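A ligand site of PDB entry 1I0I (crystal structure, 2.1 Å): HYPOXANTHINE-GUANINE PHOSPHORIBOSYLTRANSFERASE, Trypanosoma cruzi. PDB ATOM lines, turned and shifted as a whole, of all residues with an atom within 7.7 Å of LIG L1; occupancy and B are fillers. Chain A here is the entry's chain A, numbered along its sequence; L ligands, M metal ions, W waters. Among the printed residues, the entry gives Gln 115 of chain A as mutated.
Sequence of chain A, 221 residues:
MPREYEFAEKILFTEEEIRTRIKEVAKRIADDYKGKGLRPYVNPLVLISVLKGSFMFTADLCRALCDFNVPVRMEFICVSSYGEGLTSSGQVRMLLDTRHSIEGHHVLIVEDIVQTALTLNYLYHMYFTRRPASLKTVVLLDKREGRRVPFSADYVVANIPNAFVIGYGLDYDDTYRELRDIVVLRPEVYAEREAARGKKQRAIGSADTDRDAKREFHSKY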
ATOM      1  N   ASP A 112       6.333  24.560 -35.688  1.00  0.00           N
ATOM      2  CA  ASP A 112       5.626  24.295 -34.440  1.00  0.00           C
ATOM      3  C   ASP A 112       6.453  24.756 -33.226  1.00  0.00           C
ATOM      4  O   ASP A 112       5.933  25.382 -32.301  1.00  0.00           O
ATOM      5  CB  ASP A 112       5.265  22.803 -34.323  1.00  0.00           C
ATOM      6  CG  ASP A 112       6.468  21.860 -34.523  1.00  0.00           C
ATOM      7  OD1 ASP A 112       7.577  22.288 -34.941  1.00  0.00           O
ATOM      8  OD2 ASP A 112       6.291  20.641 -34.277  1.00  0.00           O
ATOM      9  N   ILE A 113       7.747  24.472 -33.248  1.00  0.00           N
ATOM     10  CA  ILE A 113       8.620  24.841 -32.151  1.00  0.00           C
ATOM     11  C   ILE A 113      10.063  25.058 -32.591  1.00  0.00           C
ATOM     12  O   ILE A 113      10.523  24.498 -33.599  1.00  0.00           O
ATOM     13  CB  ILE A 113       8.568  23.799 -31.001  1.00  0.00           C
ATOM     14  CG1 ILE A 113       9.307  24.331 -29.762  1.00  0.00           C
ATOM     15  CG2 ILE A 113       9.147  22.460 -31.461  1.00  0.00           C
ATOM     16  CD1 ILE A 113       8.843  23.712 -28.434  1.00  0.00           C
ATOM     17  N   VAL A 114      10.741  25.956 -31.874  1.00  0.00           N
ATOM     18  CA  VAL A 114      12.143  26.257 -32.126  1.00  0.00           C
ATOM     19  C   VAL A 114      12.822  26.256 -30.765  1.00  0.00           C
ATOM     20  O   VAL A 114      12.248  26.693 -29.765  1.00  0.00           O
ATOM     21  CB  VAL A 114      12.339  27.628 -32.858  1.00  0.00           C
ATOM     22  CG1 VAL A 114      11.753  28.802 -32.052  1.00  0.00           C
ATOM     23  CG2 VAL A 114      13.816  27.852 -33.133  1.00  0.00           C
ATOM     24  N   GLN A 115      13.982  25.622 -30.720  1.00  0.00           N
ATOM     25  CA  GLN A 115      14.769  25.559 -29.503  1.00  0.00           C
ATOM     26  C   GLN A 115      16.221  25.876 -29.853  1.00  0.00           C
ATOM     27  O   GLN A 115      16.676  27.009 -29.644  1.00  0.00           O
ATOM     28  CB  GLN A 115      14.656  24.200 -28.813  1.00  0.00           C
ATOM     29  CG  GLN A 115      15.500  24.118 -27.540  1.00  0.00           C
ATOM     30  CD  GLN A 115      15.214  22.889 -26.702  1.00  0.00           C
ATOM     31  OE1 GLN A 115      14.684  21.884 -27.178  1.00  0.00           O
ATOM     32  NE2 GLN A 115      15.545  22.978 -25.412  1.00  0.00           N
ATOM     33  N   THR A 116      16.929  24.891 -30.402  1.00  0.00           N
ATOM     34  CA  THR A 116      18.311  25.091 -30.818  1.00  0.00           C
ATOM     35  C   THR A 116      18.383  25.998 -32.033  1.00  0.00           C
ATOM     36  O   THR A 116      19.373  26.701 -32.245  1.00  0.00           O
ATOM     37  CB  THR A 116      19.013  23.764 -31.150  1.00  0.00           C
ATOM     38  OG1 THR A 116      18.501  23.230 -32.367  1.00  0.00           O
ATOM     39  CG2 THR A 116      18.779  22.758 -30.033  1.00  0.00           C
ATOM     40  N   LEU A 141       5.678  27.628 -30.640  1.00  0.00           N
ATOM     41  CA  LEU A 141       6.293  27.698 -29.321  1.00  0.00           C
ATOM     42  C   LEU A 141       7.756  28.035 -29.441  1.00  0.00           C
ATOM     43  O   LEU A 141       8.429  27.552 -30.346  1.00  0.00           O
ATOM     44  CB  LEU A 141       6.147  26.365 -28.596  1.00  0.00           C
ATOM     45  CG  LEU A 141       4.726  25.794 -28.435  1.00  0.00           C
ATOM     46  CD1 LEU A 141       4.824  24.400 -27.848  1.00  0.00           C
ATOM     47  CD2 LEU A 141       3.870  26.670 -27.544  1.00  0.00           C
ATOM     48  N   LYS A 143      11.300  28.134 -27.288  1.00  0.00           N
ATOM     49  CA  LYS A 143      12.131  27.843 -26.123  1.00  0.00           C
ATOM     50  C   LYS A 143      13.361  28.721 -26.388  1.00  0.00           C
ATOM     51  O   LYS A 143      14.389  28.258 -26.871  1.00  0.00           O
ATOM     52  CB  LYS A 143      12.525  26.369 -26.078  1.00  0.00           C
ATOM     53  CG  LYS A 143      11.440  25.433 -25.599  1.00  0.00           C
ATOM     54  CD  LYS A 143      11.959  23.996 -25.614  1.00  0.00           C
ATOM     55  CE  LYS A 143      10.895  22.993 -25.224  1.00  0.00           C
ATOM     56  NZ  LYS A 143      11.434  21.623 -25.195  1.00  0.00           N
ATOM     57  N   ILE A 160       8.088  29.466 -24.146  1.00  0.00           N
ATOM     58  CA  ILE A 160       7.931  28.464 -23.095  1.00  0.00           C
ATOM     59  C   ILE A 160       9.282  28.037 -22.557  1.00  0.00           C
ATOM     60  O   ILE A 160      10.323  28.383 -23.136  1.00  0.00           O
ATOM     61  CB  ILE A 160       7.183  27.168 -23.614  1.00  0.00           C
ATOM     62  CG1 ILE A 160       7.985  26.489 -24.710  1.00  0.00           C
ATOM     63  CG2 ILE A 160       5.775  27.493 -24.127  1.00  0.00           C
ATOM     64  CD1 ILE A 160       7.505  25.064 -25.013  1.00  0.00           C
ATOM     65  N   PRO A 161       9.280  27.394 -21.376  1.00  0.00           N
ATOM     66  CA  PRO A 161      10.563  26.952 -20.807  1.00  0.00           C
ATOM     67  C   PRO A 161      10.917  25.597 -21.409  1.00  0.00           C
ATOM     68  O   PRO A 161      10.119  25.007 -22.161  1.00  0.00           O
ATOM     69  CB  PRO A 161      10.256  26.874 -19.314  1.00  0.00           C
ATOM     70  CG  PRO A 161       8.791  26.512 -19.301  1.00  0.00           C
ATOM     71  CD  PRO A 161       8.202  27.360 -20.373  1.00  0.00           C
ATOM     72  N   ASN A 162      12.115  25.101 -21.090  1.00  0.00           N
ATOM     73  CA  ASN A 162      12.547  23.824 -21.641  1.00  0.00           C
ATOM     74  C   ASN A 162      11.900  22.547 -21.070  1.00  0.00           C
ATOM     75  O   ASN A 162      12.572  21.666 -20.520  1.00  0.00           O
ATOM     76  CB  ASN A 162      14.072  23.684 -21.597  1.00  0.00           C
ATOM     77  CG  ASN A 162      14.562  22.545 -22.462  1.00  0.00           C
ATOM     78  OD1 ASN A 162      13.959  22.212 -23.475  1.00  0.00           O
ATOM     79  ND2 ASN A 162      15.648  21.915 -22.051  1.00  0.00           N
ATOM     80  N   ALA A 163      10.590  22.454 -21.212  1.00  0.00           N
ATOM     81  CA  ALA A 163       9.832  21.296 -20.793  1.00  0.00           C
ATOM     82  C   ALA A 163       9.617  20.482 -22.081  1.00  0.00           C
ATOM     83  O   ALA A 163       9.767  21.026 -23.178  1.00  0.00           O
ATOM     84  CB  ALA A 163       8.500  21.732 -20.229  1.00  0.00           C
ATOM     85  N   PHE A 164       9.378  19.175 -21.973  1.00  0.00           N
ATOM     86  CA  PHE A 164       9.098  18.413 -23.208  1.00  0.00           C
ATOM     87  C   PHE A 164       7.603  18.453 -23.403  1.00  0.00           C
ATOM     88  O   PHE A 164       6.831  17.915 -22.597  1.00  0.00           O
ATOM     89  CB  PHE A 164       9.575  16.951 -23.206  1.00  0.00           C
ATOM     90  CG  PHE A 164       9.649  16.375 -24.609  1.00  0.00           C
ATOM     91  CD1 PHE A 164      10.662  16.780 -25.483  1.00  0.00           C
ATOM     92  CD2 PHE A 164       8.657  15.530 -25.083  1.00  0.00           C
ATOM     93  CE1 PHE A 164      10.671  16.348 -26.830  1.00  0.00           C
ATOM     94  CE2 PHE A 164       8.659  15.099 -26.423  1.00  0.00           C
ATOM     95  CZ  PHE A 164       9.676  15.511 -27.292  1.00  0.00           C
ATOM     96  N   VAL A 165       7.206  19.180 -24.446  1.00  0.00           N
ATOM     97  CA  VAL A 165       5.808  19.372 -24.785  1.00  0.00           C
ATOM     98  C   VAL A 165       5.355  18.459 -25.904  1.00  0.00           C
ATOM     99  O   VAL A 165       6.132  18.094 -26.782  1.00  0.00           O
ATOM    100  CB  VAL A 165       5.511  20.854 -25.154  1.00  0.00           C
ATOM    101  CG1 VAL A 165       5.753  21.737 -23.938  1.00  0.00           C
ATOM    102  CG2 VAL A 165       6.380  21.296 -26.315  1.00  0.00           C
ATOM    103  N   ILE A 166       4.082  18.105 -25.851  1.00  0.00           N
ATOM    104  CA  ILE A 166       3.458  17.222 -26.818  1.00  0.00           C
ATOM    105  C   ILE A 166       2.035  17.708 -27.077  1.00  0.00           C
ATOM    106  O   ILE A 166       1.447  18.414 -26.246  1.00  0.00           O
ATOM    107  CB  ILE A 166       3.401  15.761 -26.282  1.00  0.00           C
ATOM    108  CG1 ILE A 166       2.850  15.753 -24.855  1.00  0.00           C
ATOM    109  CG2 ILE A 166       4.777  15.114 -26.336  1.00  0.00           C
ATOM    110  CD1 ILE A 166       2.684  14.381 -24.259  1.00  0.00           C
ATOM    111  N   GLY A 167       1.493  17.303 -28.210  1.00  0.00           N
ATOM    112  CA  GLY A 167       0.154  17.703 -28.573  1.00  0.00           C
ATOM    113  C   GLY A 167       0.192  18.769 -29.619  1.00  0.00           C
ATOM    114  O   GLY A 167       1.256  19.355 -29.897  1.00  0.00           O
ATOM    115  N   GLY A 169       0.305  18.715 -32.876  1.00  0.00           N
ATOM    116  CA  GLY A 169       1.318  18.495 -33.886  1.00  0.00           C
ATOM    117  C   GLY A 169       2.664  18.034 -33.332  1.00  0.00           C
ATOM    118  O   GLY A 169       3.391  17.328 -34.012  1.00  0.00           O
ATOM    119  N   LEU A 170       2.964  18.440 -32.097  1.00  0.00           N
ATOM    120  CA  LEU A 170       4.190  18.100 -31.392  1.00  0.00           C
ATOM    121  C   LEU A 170       4.160  16.669 -30.890  1.00  0.00           C
ATOM    122  O   LEU A 170       3.228  16.265 -30.186  1.00  0.00           O
ATOM    123  CB  LEU A 170       4.364  19.048 -30.206  1.00  0.00           C
ATOM    124  CG  LEU A 170       4.643  20.505 -30.586  1.00  0.00           C
ATOM    125  CD1 LEU A 170       4.252  21.435 -29.460  1.00  0.00           C
ATOM    126  CD2 LEU A 170       6.107  20.646 -30.910  1.00  0.00           C
ATOM    127  N   ASP A 171       5.229  15.936 -31.125  1.00  0.00           N
ATOM    128  CA  ASP A 171       5.267  14.535 -30.719  1.00  0.00           C
ATOM    129  C   ASP A 171       6.397  14.142 -29.792  1.00  0.00           C
ATOM    130  O   ASP A 171       7.394  14.852 -29.621  1.00  0.00           O
ATOM    131  CB  ASP A 171       5.443  13.656 -31.953  1.00  0.00           C
ATOM    132  CG  ASP A 171       6.858  13.734 -32.529  1.00  0.00           C
ATOM    133  OD1 ASP A 171       7.265  14.822 -32.981  1.00  0.00           O
ATOM    134  OD2 ASP A 171       7.590  12.722 -32.514  1.00  0.00           O
ATOM    135  N   TYR A 172       6.248  12.941 -29.265  1.00  0.00           N
ATOM    136  CA  TYR A 172       7.285  12.297 -28.488  1.00  0.00           C
ATOM    137  C   TYR A 172       7.278  10.909 -29.108  1.00  0.00           C
ATOM    138  O   TYR A 172       6.292  10.191 -28.983  1.00  0.00           O
ATOM    139  CB  TYR A 172       6.963  12.146 -27.016  1.00  0.00           C
ATOM    140  CG  TYR A 172       7.946  11.170 -26.408  1.00  0.00           C
ATOM    141  CD1 TYR A 172       9.298  11.498 -26.315  1.00  0.00           C
ATOM    142  CD2 TYR A 172       7.546   9.889 -26.027  1.00  0.00           C
ATOM    143  CE1 TYR A 172      10.225  10.572 -25.876  1.00  0.00           C
ATOM    144  CE2 TYR A 172       8.465   8.951 -25.580  1.00  0.00           C
ATOM    145  CZ  TYR A 172       9.800   9.292 -25.510  1.00  0.00           C
ATOM    146  OH  TYR A 172      10.721   8.372 -25.094  1.00  0.00           O
ATOM    147  N   ARG A 177       0.787  13.647 -31.425  1.00  0.00           N
ATOM    148  CA  ARG A 177       0.646  14.808 -32.325  1.00  0.00           C
ATOM    149  C   ARG A 177      -0.809  15.241 -32.471  1.00  0.00           C
ATOM    150  O   ARG A 177      -1.091  16.406 -32.725  1.00  0.00           O
ATOM    151  CB  ARG A 177       1.112  14.494 -33.739  1.00  0.00           C
ATOM    152  CG  ARG A 177       2.541  14.062 -33.904  1.00  0.00           C
ATOM    153  CD  ARG A 177       2.907  14.152 -35.392  1.00  0.00           C
ATOM    154  NE  ARG A 177       4.241  13.629 -35.658  1.00  0.00           N
ATOM    155  CZ  ARG A 177       5.381  14.301 -35.513  1.00  0.00           C
ATOM    156  NH1 ARG A 177       5.387  15.566 -35.062  1.00  0.00           N
ATOM    157  NH2 ARG A 177       6.526  13.684 -35.754  1.00  0.00           N
ATOM    158  N   VAL A 183       0.597  19.855 -23.869  1.00  0.00           N
ATOM    159  CA  VAL A 183       0.845  19.429 -22.503  1.00  0.00           C
ATOM    160  C   VAL A 183       2.313  19.028 -22.314  1.00  0.00           C
ATOM    161  O   VAL A 183       3.054  18.855 -23.281  1.00  0.00           O
ATOM    162  CB  VAL A 183      -0.093  18.219 -22.134  1.00  0.00           C
ATOM    163  CG1 VAL A 183      -1.551  18.574 -22.367  1.00  0.00           C
ATOM    164  CG2 VAL A 183       0.271  16.965 -22.944  1.00  0.00           C
ATOM    165  N   LEU A 185       5.019  16.297 -21.157  1.00  0.00           N
ATOM    166  CA  LEU A 185       5.172  14.864 -21.031  1.00  0.00           C
ATOM    167  C   LEU A 185       5.727  14.480 -19.648  1.00  0.00           C
ATOM    168  O   LEU A 185       6.740  15.024 -19.196  1.00  0.00           O
ATOM    169  CB  LEU A 185       6.098  14.362 -22.147  1.00  0.00           C
ATOM    170  CG  LEU A 185       6.412  12.875 -22.275  1.00  0.00           C
ATOM    171  CD1 LEU A 185       5.165  12.091 -22.703  1.00  0.00           C
ATOM    172  CD2 LEU A 185       7.536  12.694 -23.268  1.00  0.00           C
HETATM  173  C1  LIG L   1      11.495  19.688 -30.333  1.00  0.00           C
HETATM  174  C2  LIG L   1      10.440  19.172 -29.540  1.00  0.00           C
HETATM  175  N1  LIG L   1       9.429  18.361 -29.962  1.00  0.00           N
HETATM  176  C3  LIG L   1       8.426  18.315 -29.040  1.00  0.00           C
HETATM  177  N2  LIG L   1       8.526  18.867 -27.801  1.00  0.00           N
HETATM  178  C4  LIG L   1       9.568  19.596 -27.327  1.00  0.00           C
HETATM  179  O1  LIG L   1       9.520  20.053 -26.188  1.00  0.00           O
HETATM  180  C5  LIG L   1      10.587  19.743 -28.294  1.00  0.00           C
HETATM  181  N3  LIG L   1      11.813  20.407 -28.249  1.00  0.00           N
HETATM  182  N4  LIG L   1      12.270  20.395 -29.486  1.00  0.00           N
HETATM  183  C1  LG2 L   2      11.254  19.216 -33.994  1.00  0.00           C
HETATM  184  C2  LG2 L   2      10.179  20.256 -33.907  1.00  0.00           C
HETATM  185  C3  LG2 L   2      10.925  21.394 -34.619  1.00  0.00           C
HETATM  186  C4  LG2 L   2      12.354  21.307 -34.135  1.00  0.00           C
HETATM  187  C5  LG2 L   2      12.474  22.052 -32.792  1.00  0.00           C
HETATM  188  O1  LG2 L   2      10.931  18.453 -35.184  1.00  0.00           O
HETATM  189  O2  LG2 L   2       9.015  19.739 -34.622  1.00  0.00           O
HETATM  190  O3  LG2 L   2      11.191  21.147 -35.970  1.00  0.00           O
HETATM  191  O4  LG2 L   2      12.543  19.880 -34.076  1.00  0.00           O
HETATM  192  O5  LG2 L   2      13.750  21.893 -32.166  1.00  0.00           O
HETATM  193  P1  LG2 L   2      15.106  22.663 -32.671  1.00  0.00           P
HETATM  194  O6  LG2 L   2      14.767  24.088 -32.908  1.00  0.00           O
HETATM  195  O7  LG2 L   2      15.516  21.881 -33.876  1.00  0.00           O
HETATM  196  O8  LG2 L   2      16.012  22.552 -31.523  1.00  0.00           O
HETATM  197  P2  LG2 L   2      11.282  16.952 -35.453  1.00  0.00           P
HETATM  198  O9  LG2 L   2      12.713  16.925 -35.759  1.00  0.00           O
HETATM  199  O10 LG2 L   2      10.947  16.313 -34.186  1.00  0.00           O
HETATM  200  O11 LG2 L   2      10.436  16.641 -36.667  1.00  0.00           O
HETATM  201  P3  LG2 L   2       8.941  16.521 -36.743  1.00  0.00           P
HETATM  202  O12 LG2 L   2       8.403  15.822 -35.553  1.00  0.00           O
HETATM  203  O13 LG2 L   2       8.582  15.780 -37.950  1.00  0.00           O
HETATM  204  O14 LG2 L   2       8.313  17.899 -36.818  1.00  0.00           O
HETATM  205 MG    MG M   1       9.147  15.409 -33.393  1.00  0.00          MG
HETATM  206 MG    MG M   2       9.243  19.772 -37.018  1.00  0.00          MG
HETATM  207  O   HOH W   1       8.298  17.279 -32.963  1.00  0.00           O
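An oxygen (O1) of LIG L1 lies within hydrogen-bond range of the side-chain amino group (NZ) of Lys 143, 2.7 Å away. The backbone NH of Val 165 is in hydrogen-bond range of an oxygen (O1) of LIG L1. N2 of LIG L1 lies close to O of Val 165, at 2.7 Å. The backbone carbonyl oxygen (O) of Ala 163 lies within hydrogen-bond range of an oxygen (O1) of LIG L1, 3.2 Å away. N3 of LIG L1 lies within hydrogen-bond range of OE1 of Gln 115, at 3.4 Å. An oxygen (O6) of LG2 L2 lies within hydrogen-bond range of the backbone NH of Gln 115 (2.8 Å). The side-chain carboxylate (OD2) of Asp 112 sits close to an oxygen (O2) of LG2 L2, at 2.9 Å. The backbone NH (N) of Thr 116 lies within hydrogen-bond range of an oxygen (O8) of LG2 L2 (2.8 Å). The side-chain hydroxyl of Thr 116 lies within hydrogen-bond range of an oxygen (O8) of LG2 L2 (2.7 Å). The guanidinium group (NH2) of Arg 177 is in salt-bridge range of an oxygen (O13) of LG2 L2, at 3.7 Å.
The side-chain amino group (NZ) of Lys 143 lies within hydrogen-bond range of the backbone carbonyl oxygen (O) of Ala 163, at 2.7 Å. OD1 of Asn 162 is in hydrogen-bond range of NZ of Lys 143. O of Val 114 is in hydrogen-bond range of N of Lys 143. NE2 of Gln 115 is in hydrogen-bond range of OD1 of Asn 162 (2.6 Å). O of Phe 164 lies within hydrogen-bond range of N of Leu 185, at 2.8 Å. NH2 of Arg 177 is in salt-bridge range of OD2 of Asp 171 (3.5 Å).
Residues that only touch LIG L1: Ile 113, Phe 164, Leu 170 and Asp 171. Of the 22 residues printed, 8 come within 4 Å of LIG L1. The nearest printed residue that does not touch LIG L1 is Ile 166 (4.9 Å).
An oxygen (O5) of LG2 L2 sits close to a nitrogen (N4) of LIG L1 (3.4 Å).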
